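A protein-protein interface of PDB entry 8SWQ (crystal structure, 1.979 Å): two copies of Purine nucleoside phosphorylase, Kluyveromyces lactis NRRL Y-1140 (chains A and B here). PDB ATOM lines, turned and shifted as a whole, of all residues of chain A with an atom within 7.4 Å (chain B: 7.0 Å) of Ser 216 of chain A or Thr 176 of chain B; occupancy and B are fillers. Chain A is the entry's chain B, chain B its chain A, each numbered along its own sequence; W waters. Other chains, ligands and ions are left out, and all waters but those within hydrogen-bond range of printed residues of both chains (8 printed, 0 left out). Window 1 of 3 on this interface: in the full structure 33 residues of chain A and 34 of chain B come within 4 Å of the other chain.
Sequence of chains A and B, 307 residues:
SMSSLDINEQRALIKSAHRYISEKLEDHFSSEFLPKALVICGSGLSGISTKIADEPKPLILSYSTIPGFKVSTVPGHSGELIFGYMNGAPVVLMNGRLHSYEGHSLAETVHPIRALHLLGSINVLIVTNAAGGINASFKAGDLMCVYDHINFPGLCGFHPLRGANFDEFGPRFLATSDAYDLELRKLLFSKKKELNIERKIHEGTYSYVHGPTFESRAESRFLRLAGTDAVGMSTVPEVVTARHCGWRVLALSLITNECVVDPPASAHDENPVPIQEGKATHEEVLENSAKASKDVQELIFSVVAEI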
ATOM      1  N   ILE A 134       3.614  21.695   2.070  1.00  0.00           N
ATOM      2  CA  ILE A 134       2.666  21.123   3.030  1.00  0.00           C
ATOM      3  C   ILE A 134       3.395  20.423   4.177  1.00  0.00           C
ATOM      4  O   ILE A 134       2.991  20.518   5.337  1.00  0.00           O
ATOM      5  CB  ILE A 134       1.699  20.135   2.322  1.00  0.00           C
ATOM      6  CG1 ILE A 134       0.724  20.907   1.413  1.00  0.00           C
ATOM      7  CG2 ILE A 134       0.894  19.349   3.333  1.00  0.00           C
ATOM      8  CD1 ILE A 134      -0.446  21.599   2.189  1.00  0.00           C
ATOM      9  N   THR A 213      -8.263  28.481  -6.240  1.00  0.00           N
ATOM     10  CA  THR A 213      -8.001  29.062  -4.920  1.00  0.00           C
ATOM     11  C   THR A 213      -6.775  28.440  -4.280  1.00  0.00           C
ATOM     12  O   THR A 213      -6.495  27.262  -4.479  1.00  0.00           O
ATOM     13  CB  THR A 213      -9.179  28.853  -3.965  1.00  0.00           C
ATOM     14  OG1 THR A 213      -9.600  27.482  -4.042  1.00  0.00           O
ATOM     15  CG2 THR A 213     -10.347  29.766  -4.347  1.00  0.00           C
ATOM     16  N   PHE A 214      -6.043  29.227  -3.495  1.00  0.00           N
ATOM     17  CA  PHE A 214      -5.072  28.632  -2.582  1.00  0.00           C
ATOM     18  C   PHE A 214      -5.841  27.947  -1.452  1.00  0.00           C
ATOM     19  O   PHE A 214      -6.979  28.338  -1.129  1.00  0.00           O
ATOM     20  CB  PHE A 214      -4.120  29.699  -2.026  1.00  0.00           C
ATOM     21  CG  PHE A 214      -3.201  30.288  -3.061  1.00  0.00           C
ATOM     22  CD1 PHE A 214      -2.151  29.531  -3.587  1.00  0.00           C
ATOM     23  CD2 PHE A 214      -3.370  31.605  -3.494  1.00  0.00           C
ATOM     24  CE1 PHE A 214      -1.286  30.080  -4.547  1.00  0.00           C
ATOM     25  CE2 PHE A 214      -2.520  32.153  -4.449  1.00  0.00           C
ATOM     26  CZ  PHE A 214      -1.474  31.385  -4.976  1.00  0.00           C
ATOM     27  N   GLU A 215      -5.226  26.937  -0.843  1.00  0.00           N
ATOM     28  CA  GLU A 215      -5.895  26.109   0.161  1.00  0.00           C
ATOM     29  C   GLU A 215      -6.215  26.870   1.454  1.00  0.00           C
ATOM     30  O   GLU A 215      -5.447  27.725   1.889  1.00  0.00           O
ATOM     31  CB  GLU A 215      -5.030  24.882   0.498  1.00  0.00           C
ATOM     32  CG  GLU A 215      -4.751  23.945  -0.698  1.00  0.00           C
ATOM     33  CD  GLU A 215      -3.845  24.562  -1.764  1.00  0.00           C
ATOM     34  OE1 GLU A 215      -3.990  24.184  -2.952  1.00  0.00           O
ATOM     35  OE2 GLU A 215      -2.998  25.440  -1.435  1.00  0.00           O
ATOM     36  N   SER A 216      -7.353  26.539   2.056  1.00  0.00           N
ATOM     37  CA  SER A 216      -7.716  27.040   3.374  1.00  0.00           C
ATOM     38  C   SER A 216      -6.821  26.353   4.389  1.00  0.00           C
ATOM     39  O   SER A 216      -6.098  25.415   4.058  1.00  0.00           O
ATOM     40  CB  SER A 216      -9.188  26.729   3.681  1.00  0.00           C
ATOM     41  OG  SER A 216      -9.382  25.331   3.885  1.00  0.00           O
ATOM     42  N   ARG A 217      -6.830  26.836   5.622  1.00  0.00           N
ATOM     43  CA  ARG A 217      -5.993  26.235   6.656  1.00  0.00           C
ATOM     44  C   ARG A 217      -6.408  24.792   6.863  1.00  0.00           C
ATOM     45  O   ARG A 217      -5.555  23.903   6.932  1.00  0.00           O
ATOM     46  CB  ARG A 217      -6.136  27.013   7.970  1.00  0.00           C
ATOM     47  CG  ARG A 217      -5.813  28.484   7.790  1.00  0.00           C
ATOM     48  CD  ARG A 217      -6.606  29.367   8.757  1.00  0.00           C
ATOM     49  NE  ARG A 217      -6.259  30.772   8.543  1.00  0.00           N
ATOM     50  CZ  ARG A 217      -5.256  31.398   9.141  1.00  0.00           C
ATOM     51  NH1 ARG A 217      -4.499  30.749  10.019  1.00  0.00           N
ATOM     52  NH2 ARG A 217      -5.012  32.675   8.862  1.00  0.00           N
ATOM     53  N   ALA A 218      -7.716  24.550   6.968  1.00  0.00           N
ATOM     54  CA  ALA A 218      -8.191  23.181   7.186  1.00  0.00           C
ATOM     55  C   ALA A 218      -7.890  22.266   6.007  1.00  0.00           C
ATOM     56  O   ALA A 218      -7.585  21.071   6.188  1.00  0.00           O
ATOM     57  CB  ALA A 218      -9.687  23.159   7.514  1.00  0.00           C
ATOM     58  N   GLU A 219      -7.979  22.810   4.800  1.00  0.00           N
ATOM     59  CA  GLU A 219      -7.638  22.035   3.601  1.00  0.00           C
ATOM     60  C   GLU A 219      -6.163  21.639   3.614  1.00  0.00           C
ATOM     61  O   GLU A 219      -5.814  20.505   3.311  1.00  0.00           O
ATOM     62  CB  GLU A 219      -7.952  22.827   2.328  1.00  0.00           C
ATOM     63  CG  GLU A 219      -9.428  22.829   1.965  1.00  0.00           C
ATOM     64  CD  GLU A 219      -9.827  23.940   1.005  1.00  0.00           C
ATOM     65  OE1 GLU A 219      -8.947  24.664   0.487  1.00  0.00           O
ATOM     66  OE2 GLU A 219     -11.051  24.112   0.772  1.00  0.00           O
ATOM     67  N   SER A 220      -5.290  22.574   3.952  1.00  0.00           N
ATOM     68  CA  SER A 220      -3.862  22.252   4.035  1.00  0.00           C
ATOM     69  C   SER A 220      -3.533  21.250   5.136  1.00  0.00           C
ATOM     70  O   SER A 220      -2.644  20.408   4.961  1.00  0.00           O
ATOM     71  CB  SER A 220      -3.037  23.531   4.224  1.00  0.00           C
ATOM     72  OG  SER A 220      -3.121  24.299   3.033  1.00  0.00           O
ATOM     73  N   ARG A 221      -4.207  21.336   6.284  1.00  0.00           N
ATOM     74  CA  ARG A 221      -4.012  20.314   7.315  1.00  0.00           C
ATOM     75  C   ARG A 221      -4.514  18.952   6.837  1.00  0.00           C
ATOM     76  O   ARG A 221      -3.920  17.907   7.155  1.00  0.00           O
ATOM     77  CB  ARG A 221      -4.700  20.677   8.646  1.00  0.00           C
ATOM     78  CG  ARG A 221      -4.076  21.854   9.382  1.00  0.00           C
ATOM     79  CD  ARG A 221      -4.540  21.925  10.836  1.00  0.00           C
ATOM     80  NE  ARG A 221      -5.996  21.897  10.945  1.00  0.00           N
ATOM     81  CZ  ARG A 221      -6.771  22.971  10.850  1.00  0.00           C
ATOM     82  NH1 ARG A 221      -6.234  24.177  10.654  1.00  0.00           N
ATOM     83  NH2 ARG A 221      -8.081  22.841  10.975  1.00  0.00           N
ATOM     84  N   PHE A 222      -5.641  18.961   6.130  1.00  0.00           N
ATOM     85  CA  PHE A 222      -6.143  17.741   5.487  1.00  0.00           C
ATOM     86  C   PHE A 222      -5.098  17.127   4.542  1.00  0.00           C
ATOM     87  O   PHE A 222      -4.760  15.934   4.651  1.00  0.00           O
ATOM     88  CB  PHE A 222      -7.456  18.005   4.736  1.00  0.00           C
ATOM     89  CG  PHE A 222      -7.809  16.918   3.753  1.00  0.00           C
ATOM     90  CD1 PHE A 222      -8.169  15.654   4.203  1.00  0.00           C
ATOM     91  CD2 PHE A 222      -7.754  17.154   2.382  1.00  0.00           C
ATOM     92  CE1 PHE A 222      -8.484  14.636   3.313  1.00  0.00           C
ATOM     93  CE2 PHE A 222      -8.060  16.134   1.471  1.00  0.00           C
ATOM     94  CZ  PHE A 222      -8.425  14.870   1.943  1.00  0.00           C
ATOM     95  N   LEU A 223      -4.574  17.934   3.618  1.00  0.00           N
ATOM     96  CA  LEU A 223      -3.553  17.450   2.690  1.00  0.00           C
ATOM     97  C   LEU A 223      -2.346  16.872   3.411  1.00  0.00           C
ATOM     98  O   LEU A 223      -1.779  15.868   2.987  1.00  0.00           O
ATOM     99  CB  LEU A 223      -3.126  18.575   1.731  1.00  0.00           C
ATOM    100  CG  LEU A 223      -4.260  19.043   0.807  1.00  0.00           C
ATOM    101  CD1 LEU A 223      -3.897  20.382   0.140  1.00  0.00           C
ATOM    102  CD2 LEU A 223      -4.557  17.978  -0.257  1.00  0.00           C
ATOM    103  N   CYS A 259       2.362  26.590   3.087  1.00  0.00           N
ATOM    104  CA  CYS A 259       0.909  26.672   3.214  1.00  0.00           C
ATOM    105  C   CYS A 259       0.508  26.961   4.646  1.00  0.00           C
ATOM    106  O   CYS A 259       1.057  26.363   5.574  1.00  0.00           O
ATOM    107  CB  CYS A 259       0.249  25.369   2.756  1.00  0.00           C
ATOM    108  SG  CYS A 259       0.650  24.962   1.032  1.00  0.00           S
ATOM    109  N   VAL A 260      -0.450  27.872   4.821  1.00  0.00           N
ATOM    110  CA  VAL A 260      -0.916  28.220   6.163  1.00  0.00           C
ATOM    111  C   VAL A 260      -1.754  27.077   6.726  1.00  0.00           C
ATOM    112  O   VAL A 260      -2.713  26.641   6.089  1.00  0.00           O
ATOM    113  CB  VAL A 260      -1.763  29.505   6.151  1.00  0.00           C
ATOM    114  CG1 VAL A 260      -2.160  29.893   7.594  1.00  0.00           C
ATOM    115  CG2 VAL A 260      -0.981  30.632   5.480  1.00  0.00           C
ATOM    116  N   VAL A 261      -1.392  26.586   7.911  1.00  0.00           N
ATOM    117  CA  VAL A 261      -2.107  25.456   8.524  1.00  0.00           C
ATOM    118  C   VAL A 261      -2.732  25.767   9.882  1.00  0.00           C
ATOM    119  O   VAL A 261      -3.638  25.064  10.320  1.00  0.00           O
ATOM    120  CB  VAL A 261      -1.195  24.219   8.721  1.00  0.00           C
ATOM    121  CG1 VAL A 261      -0.946  23.501   7.395  1.00  0.00           C
ATOM    122  CG2 VAL A 261       0.122  24.617   9.411  1.00  0.00           C
ATOM    123  N   ASP A 262      -2.226  26.785  10.568  1.00  0.00           N
ATOM    124  CA  ASP A 262      -2.733  27.103  11.897  1.00  0.00           C
ATOM    125  C   ASP A 262      -4.194  27.481  11.822  1.00  0.00           C
ATOM    126  O   ASP A 262      -4.596  28.154  10.886  1.00  0.00           O
ATOM    127  CB  ASP A 262      -1.958  28.269  12.527  1.00  0.00           C
ATOM    128  CG  ASP A 262      -0.546  27.893  12.925  1.00  0.00           C
ATOM    129  OD1 ASP A 262      -0.213  26.688  12.941  1.00  0.00           O
ATOM    130  OD2 ASP A 262       0.232  28.819  13.215  1.00  0.00           O
ATOM    131  N   ILE A 275      -5.843  37.185  10.457  1.00  0.00           N
ATOM    132  CA  ILE A 275      -6.086  36.087   9.520  1.00  0.00           C
ATOM    133  C   ILE A 275      -5.384  36.280   8.185  1.00  0.00           C
ATOM    134  O   ILE A 275      -5.185  35.310   7.436  1.00  0.00           O
ATOM    135  CB  ILE A 275      -7.607  35.807   9.307  1.00  0.00           C
ATOM    136  CG1 ILE A 275      -8.286  36.954   8.567  1.00  0.00           C
ATOM    137  CG2 ILE A 275      -8.304  35.566  10.653  1.00  0.00           C
ATOM    138  CD1 ILE A 275      -9.818  36.757   8.418  1.00  0.00           C
ATOM    139  N   LYS A 279      -0.624  34.860   4.180  1.00  0.00           N
ATOM    140  CA  LYS A 279      -1.460  34.381   3.069  1.00  0.00           C
ATOM    141  C   LYS A 279      -0.693  34.251   1.756  1.00  0.00           C
ATOM    142  O   LYS A 279       0.175  35.068   1.441  1.00  0.00           O
ATOM    143  CB  LYS A 279      -2.691  35.276   2.855  1.00  0.00           C
ATOM    144  CG  LYS A 279      -2.382  36.522   2.046  1.00  0.00           C
ATOM    145  CD  LYS A 279      -3.460  37.589   2.153  1.00  0.00           C
ATOM    146  CE  LYS A 279      -4.655  37.286   1.283  1.00  0.00           C
ATOM    147  NZ  LYS A 279      -5.465  38.529   1.059  1.00  0.00           N
ATOM    148  N   ALA A 280      -1.045  33.229   0.979  1.00  0.00           N
ATOM    149  CA  ALA A 280      -0.432  32.988  -0.326  1.00  0.00           C
ATOM    150  C   ALA A 280      -0.889  34.033  -1.342  1.00  0.00           C
ATOM    151  O   ALA A 280      -2.051  34.463  -1.316  1.00  0.00           O
ATOM    152  CB  ALA A 280      -0.811  31.579  -0.830  1.00  0.00           C
ATOM    153  N   TYR B 147     -15.442  29.625  10.903  1.00  0.00           N
ATOM    154  CA  TYR B 147     -14.203  30.398  10.789  1.00  0.00           C
ATOM    155  C   TYR B 147     -13.221  29.800   9.785  1.00  0.00           C
ATOM    156  O   TYR B 147     -12.139  30.333   9.559  1.00  0.00           O
ATOM    157  CB  TYR B 147     -13.582  30.715  12.158  1.00  0.00           C
ATOM    158  CG  TYR B 147     -12.876  29.603  12.923  1.00  0.00           C
ATOM    159  CD1 TYR B 147     -12.825  28.287  12.455  1.00  0.00           C
ATOM    160  CD2 TYR B 147     -12.237  29.892  14.127  1.00  0.00           C
ATOM    161  CE1 TYR B 147     -12.153  27.287  13.179  1.00  0.00           C
ATOM    162  CE2 TYR B 147     -11.571  28.908  14.854  1.00  0.00           C
ATOM    163  CZ  TYR B 147     -11.529  27.620  14.380  1.00  0.00           C
ATOM    164  OH  TYR B 147     -10.853  26.661  15.095  1.00  0.00           O
ATOM    165  N   ASP B 148     -13.641  28.712   9.158  1.00  0.00           N
ATOM    166  CA  ASP B 148     -12.814  28.014   8.178  1.00  0.00           C
ATOM    167  C   ASP B 148     -13.675  27.010   7.415  1.00  0.00           C
ATOM    168  O   ASP B 148     -14.765  26.638   7.852  1.00  0.00           O
ATOM    169  CB  ASP B 148     -11.680  27.272   8.878  1.00  0.00           C
ATOM    170  CG  ASP B 148     -10.506  26.974   7.942  1.00  0.00           C
ATOM    171  OD1 ASP B 148     -10.549  27.388   6.767  1.00  0.00           O
ATOM    172  OD2 ASP B 148      -9.531  26.344   8.384  1.00  0.00           O
ATOM    173  N   HIS B 149     -13.190  26.553   6.273  1.00  0.00           N
ATOM    174  CA  HIS B 149     -13.938  25.549   5.541  1.00  0.00           C
ATOM    175  C   HIS B 149     -13.045  24.530   4.863  1.00  0.00           C
ATOM    176  O   HIS B 149     -11.837  24.724   4.745  1.00  0.00           O
ATOM    177  CB  HIS B 149     -14.922  26.186   4.545  1.00  0.00           C
ATOM    178  CG  HIS B 149     -14.270  26.881   3.387  1.00  0.00           C
ATOM    179  ND1 HIS B 149     -14.640  28.145   2.989  1.00  0.00           N
ATOM    180  CD2 HIS B 149     -13.314  26.476   2.514  1.00  0.00           C
ATOM    181  CE1 HIS B 149     -13.909  28.509   1.945  1.00  0.00           C
ATOM    182  NE2 HIS B 149     -13.098  27.513   1.638  1.00  0.00           N
ATOM    183  N   ILE B 150     -13.658  23.430   4.449  1.00  0.00           N
ATOM    184  CA  ILE B 150     -13.002  22.473   3.579  1.00  0.00           C
ATOM    185  C   ILE B 150     -13.856  22.377   2.332  1.00  0.00           C
ATOM    186  O   ILE B 150     -15.057  22.093   2.414  1.00  0.00           O
ATOM    187  CB  ILE B 150     -12.854  21.088   4.254  1.00  0.00           C
ATOM    188  CG1 ILE B 150     -11.842  21.190   5.403  1.00  0.00           C
ATOM    189  CG2 ILE B 150     -12.343  20.055   3.258  1.00  0.00           C
ATOM    190  CD1 ILE B 150     -11.915  20.052   6.415  1.00  0.00           C
ATOM    191  N   ASN B 151     -13.239  22.656   1.185  1.00  0.00           N
ATOM    192  CA  ASN B 151     -13.911  22.544  -0.107  1.00  0.00           C
ATOM    193  C   ASN B 151     -13.396  21.320  -0.853  1.00  0.00           C
ATOM    194  O   ASN B 151     -12.675  21.437  -1.849  1.00  0.00           O
ATOM    195  CB  ASN B 151     -13.702  23.824  -0.931  1.00  0.00           C
ATOM    196  CG  ASN B 151     -14.572  23.871  -2.185  1.00  0.00           C
ATOM    197  OD1 ASN B 151     -15.413  22.994  -2.394  1.00  0.00           O
ATOM    198  ND2 ASN B 151     -14.389  24.920  -3.015  1.00  0.00           N
ATOM    199  N   LEU B 155     -11.314  20.808  -4.484  1.00  0.00           N
ATOM    200  CA  LEU B 155     -10.005  20.180  -4.671  1.00  0.00           C
ATOM    201  C   LEU B 155     -10.063  19.170  -5.799  1.00  0.00           C
ATOM    202  O   LEU B 155      -9.085  18.956  -6.524  1.00  0.00           O
ATOM    203  CB  LEU B 155      -9.598  19.432  -3.391  1.00  0.00           C
ATOM    204  CG  LEU B 155      -9.342  20.268  -2.145  1.00  0.00           C
ATOM    205  CD1 LEU B 155      -8.849  19.344  -1.014  1.00  0.00           C
ATOM    206  CD2 LEU B 155      -8.335  21.383  -2.443  1.00  0.00           C
ATOM    207  N   HIS B 159     -15.455  23.500  -8.892  1.00  0.00           N
ATOM    208  CA  HIS B 159     -15.071  24.745  -8.219  1.00  0.00           C
ATOM    209  C   HIS B 159     -15.797  25.906  -8.899  1.00  0.00           C
ATOM    210  O   HIS B 159     -15.863  25.963 -10.135  1.00  0.00           O
ATOM    211  CB  HIS B 159     -13.547  24.927  -8.348  1.00  0.00           C
ATOM    212  CG  HIS B 159     -12.969  25.944  -7.413  1.00  0.00           C
ATOM    213  ND1 HIS B 159     -13.266  27.288  -7.504  1.00  0.00           N
ATOM    214  CD2 HIS B 159     -12.116  25.813  -6.365  1.00  0.00           C
ATOM    215  CE1 HIS B 159     -12.623  27.944  -6.544  1.00  0.00           C
ATOM    216  NE2 HIS B 159     -11.919  27.071  -5.843  1.00  0.00           N
ATOM    217  N   LEU B 174      -7.082  33.175  -5.654  1.00  0.00           N
ATOM    218  CA  LEU B 174      -7.685  33.741  -4.459  1.00  0.00           C
ATOM    219  C   LEU B 174      -7.266  32.925  -3.243  1.00  0.00           C
ATOM    220  O   LEU B 174      -7.434  31.706  -3.229  1.00  0.00           O
ATOM    221  CB  LEU B 174      -9.210  33.701  -4.597  1.00  0.00           C
ATOM    222  CG  LEU B 174     -10.002  34.189  -3.370  1.00  0.00           C
ATOM    223  CD1 LEU B 174      -9.741  35.683  -3.112  1.00  0.00           C
ATOM    224  CD2 LEU B 174     -11.493  33.928  -3.566  1.00  0.00           C
ATOM    225  N   ALA B 175      -6.722  33.584  -2.225  1.00  0.00           N
ATOM    226  CA  ALA B 175      -6.398  32.900  -0.980  1.00  0.00           C
ATOM    227  C   ALA B 175      -7.682  32.634  -0.221  1.00  0.00           C
ATOM    228  O   ALA B 175      -8.643  33.395  -0.320  1.00  0.00           O
ATOM    229  CB  ALA B 175      -5.446  33.748  -0.117  1.00  0.00           C
ATOM    230  N   THR B 176      -7.718  31.548   0.531  1.00  0.00           N
ATOM    231  CA  THR B 176      -8.868  31.300   1.387  1.00  0.00           C
ATOM    232  C   THR B 176      -8.471  31.105   2.856  1.00  0.00           C
ATOM    233  O   THR B 176      -9.316  30.802   3.685  1.00  0.00           O
ATOM    234  CB  THR B 176      -9.750  30.113   0.883  1.00  0.00           C
ATOM    235  OG1 THR B 176      -8.961  28.918   0.794  1.00  0.00           O
ATOM    236  CG2 THR B 176     -10.331  30.421  -0.504  1.00  0.00           C
ATOM    237  N   SER B 177      -7.193  31.275   3.179  1.00  0.00           N
ATOM    238  CA  SER B 177      -6.773  31.243   4.578  1.00  0.00           C
ATOM    239  C   SER B 177      -7.305  32.456   5.375  1.00  0.00           C
ATOM    240  O   SER B 177      -7.221  32.492   6.618  1.00  0.00           O
ATOM    241  CB  SER B 177      -5.252  31.123   4.704  1.00  0.00           C
ATOM    242  OG  SER B 177      -4.572  32.212   4.081  1.00  0.00           O
ATOM    243  N   ASP B 178      -7.850  33.446   4.665  1.00  0.00           N
ATOM    244  CA  ASP B 178      -8.427  34.641   5.307  1.00  0.00           C
ATOM    245  C   ASP B 178      -9.888  34.873   4.938  1.00  0.00           C
ATOM    246  O   ASP B 178     -10.352  36.008   4.857  1.00  0.00           O
ATOM    247  CB  ASP B 178      -7.635  35.892   4.938  1.00  0.00           C
ATOM    248  CG  ASP B 178      -7.620  36.164   3.435  1.00  0.00           C
ATOM    249  OD1 ASP B 178      -7.918  35.249   2.635  1.00  0.00           O
ATOM    250  OD2 ASP B 178      -7.295  37.310   3.056  1.00  0.00           O
ATOM    251  N   ALA B 179     -10.621  33.795   4.737  1.00  0.00           N
ATOM    252  CA  ALA B 179     -11.976  33.916   4.197  1.00  0.00           C
ATOM    253  C   ALA B 179     -12.998  34.419   5.218  1.00  0.00           C
ATOM    254  O   ALA B 179     -14.001  35.020   4.838  1.00  0.00           O
ATOM    255  CB  ALA B 179     -12.424  32.572   3.589  1.00  0.00           C
ATOM    256  N   TYR B 180     -12.761  34.180   6.510  1.00  0.00           N
ATOM    257  CA  TYR B 180     -13.798  34.477   7.516  1.00  0.00           C
ATOM    258  C   TYR B 180     -13.399  35.603   8.472  1.00  0.00           C
ATOM    259  O   TYR B 180     -12.777  35.357   9.497  1.00  0.00           O
ATOM    260  CB  TYR B 180     -14.219  33.191   8.262  1.00  0.00           C
ATOM    261  CG  TYR B 180     -14.818  32.167   7.303  1.00  0.00           C
ATOM    262  CD1 TYR B 180     -16.167  32.228   6.953  1.00  0.00           C
ATOM    263  CD2 TYR B 180     -14.027  31.194   6.698  1.00  0.00           C
ATOM    264  CE1 TYR B 180     -16.722  31.329   6.053  1.00  0.00           C
ATOM    265  CE2 TYR B 180     -14.591  30.260   5.785  1.00  0.00           C
ATOM    266  CZ  TYR B 180     -15.931  30.342   5.482  1.00  0.00           C
ATOM    267  OH  TYR B 180     -16.515  29.472   4.589  1.00  0.00           O
ATOM    268  N   THR B 205     -15.122  24.548  11.635  1.00  0.00           N
ATOM    269  CA  THR B 205     -14.891  24.340  10.209  1.00  0.00           C
ATOM    270  C   THR B 205     -16.082  23.664   9.555  1.00  0.00           C
ATOM    271  O   THR B 205     -16.526  22.606   9.997  1.00  0.00           O
ATOM    272  CB  THR B 205     -13.639  23.453   9.998  1.00  0.00           C
ATOM    273  OG1 THR B 205     -12.502  24.133  10.520  1.00  0.00           O
ATOM    274  CG2 THR B 205     -13.383  23.166   8.522  1.00  0.00           C
ATOM    275  N   VAL B 239     -19.350  31.691  -0.454  1.00  0.00           N
ATOM    276  CA  VAL B 239     -18.257  32.347   0.284  1.00  0.00           C
ATOM    277  C   VAL B 239     -17.088  32.649  -0.634  1.00  0.00           C
ATOM    278  O   VAL B 239     -16.606  33.787  -0.697  1.00  0.00           O
ATOM    279  CB  VAL B 239     -17.765  31.453   1.457  1.00  0.00           C
ATOM    280  CG1 VAL B 239     -16.433  31.976   2.038  1.00  0.00           C
ATOM    281  CG2 VAL B 239     -18.824  31.409   2.553  1.00  0.00           C
ATOM    282  N   VAL B 240     -16.635  31.627  -1.361  1.00  0.00           N
ATOM    283  CA  VAL B 240     -15.523  31.792  -2.295  1.00  0.00           C
ATOM    284  C   VAL B 240     -15.802  32.876  -3.330  1.00  0.00           C
ATOM    285  O   VAL B 240     -14.930  33.699  -3.654  1.00  0.00           O
ATOM    286  CB  VAL B 240     -15.198  30.442  -3.019  1.00  0.00           C
ATOM    287  CG1 VAL B 240     -14.278  30.664  -4.224  1.00  0.00           C
ATOM    288  CG2 VAL B 240     -14.573  29.462  -2.030  1.00  0.00           C
ATOM    289  N   ARG B 243     -15.801  36.319  -1.665  1.00  0.00           N
ATOM    290  CA  ARG B 243     -14.405  36.677  -1.421  1.00  0.00           C
ATOM    291  C   ARG B 243     -13.725  37.130  -2.712  1.00  0.00           C
ATOM    292  O   ARG B 243     -12.937  38.069  -2.703  1.00  0.00           O
ATOM    293  CB  ARG B 243     -13.638  35.505  -0.786  1.00  0.00           C
ATOM    294  CG  ARG B 243     -13.982  35.246   0.690  1.00  0.00           C
ATOM    295  CD  ARG B 243     -13.719  36.478   1.549  1.00  0.00           C
ATOM    296  NE  ARG B 243     -12.291  36.814   1.572  1.00  0.00           N
ATOM    297  CZ  ARG B 243     -11.797  38.040   1.705  1.00  0.00           C
ATOM    298  NH1 ARG B 243     -12.613  39.081   1.820  1.00  0.00           N
ATOM    299  NH2 ARG B 243     -10.480  38.222   1.723  1.00  0.00           N
HETATM  300  O   HOH W   1     -10.950  26.855  -0.011  1.00  0.00           O
HETATM  301  O   HOH W   2      -7.748  36.542   0.183  1.00  0.00           O
HETATM  302  O   HOH W   3      -8.945  25.579  10.674  1.00  0.00           O
HETATM  303  O   HOH W   4      -5.159  30.247   1.138  1.00  0.00           O
HETATM  304  O   HOH W   5     -12.217  26.747  -2.548  1.00  0.00           O
HETATM  305  O   HOH W   6      -3.570  33.903   5.980  1.00  0.00           O
HETATM  306  O   HOH W   7      -8.990  29.454   6.077  1.00  0.00           O
HETATM  307  O   HOH W   8      -2.957  31.432   2.045  1.00  0.00           O
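No position is printed for both chains. Of the 25 pairs that touch across the chains among the printed residues, none has its exchanged pair printed and touching as well.
Water W8 lies within hydrogen-bond range of OG of Ser 177 of chain B and N of Ala 280 of chain A.
The side-chain hydroxyl (OG1) of Thr 213 of chain A is in hydrogen-bond range of a ring nitrogen (NE2) of His 159 of chain B, 3.0 Å away. OG1 of Thr 176 of chain B is in hydrogen-bond range of N of Ser 216 of chain A, 3.1 Å away. The backbone carbonyl oxygen (O) of Ser 177 of chain B lies within hydrogen-bond range of the guanidinium group (NE) of Arg 217 of chain A (2.8 Å). The side-chain carboxylate (OD2) of Asp 178 of chain B lies within salt-bridge range of the side-chain amino group (NZ) of Lys 279 of chain A (3.0 Å). The backbone NH of Phe 214 of chain A is in hydrogen-bond range of the backbone carbonyl oxygen of Leu 174 of chain B, at 2.9 Å. The side-chain carboxylate (OE2) of Glu 219 of chain A sits at hydrogen-bond distance from the backbone NH (N) of Asn 151 of chain B, 2.7 Å away. The backbone NH of Ala 218 of chain A sits at hydrogen-bond distance from the side-chain carboxylate of Asp 148 of chain B, at 2.9 Å.
The guanidinium group (NH1) of Arg 217 of chain A is in hydrogen-bond range of the backbone carbonyl oxygen (O) of Asp 262 of chain A, 2.7 Å away. NH2 of Arg 217 of chain A lies within hydrogen-bond range of O of Ile 275 of chain A, at 3.0 Å.
His 149 of chain B touches Ala 218 of chain A. Ala 218 of chain A touches Thr 205 of chain B. OE2 of Glu 219 of chain A touches C of Ile 150 of chain B, at 3.6 Å. O of Tyr 180 of chain B touches CD1 of Ile 275 of chain A, at 3.4 Å.
Ser 216 of chain A touches three residues of chain B. Val 261 of chain A touches none of the printed residues of chain B. Printed residues of chain A within 4 Å of Ala 175 of chain B: Lys 279 and Ala 280. Thr 176 of chain B touches just these residues of chain A: Thr 213 (3.9 Å), Phe 214 (2.8 Å), Glu 215 (3.5 Å) and Ser 216 (3.1 Å). Of the printed residues of chain A, Thr 205 of chain B touches Ala 218 (3.8 Å).
Of the 18 printed residues of chain B, 12 touch a printed residue of chain A. Hydrophobic or aromatic side chains of chain B within 4 Å of the printed part of chain A: His 149, Ile 150, His 159 and Ala 175. Among the printed residues, Asp or Glu carboxylates within 4 Å of a Lys or Arg side-chain nitrogen of the other chain: Lys 279 of chain A with Asp 178 of chain B (3.0 Å).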
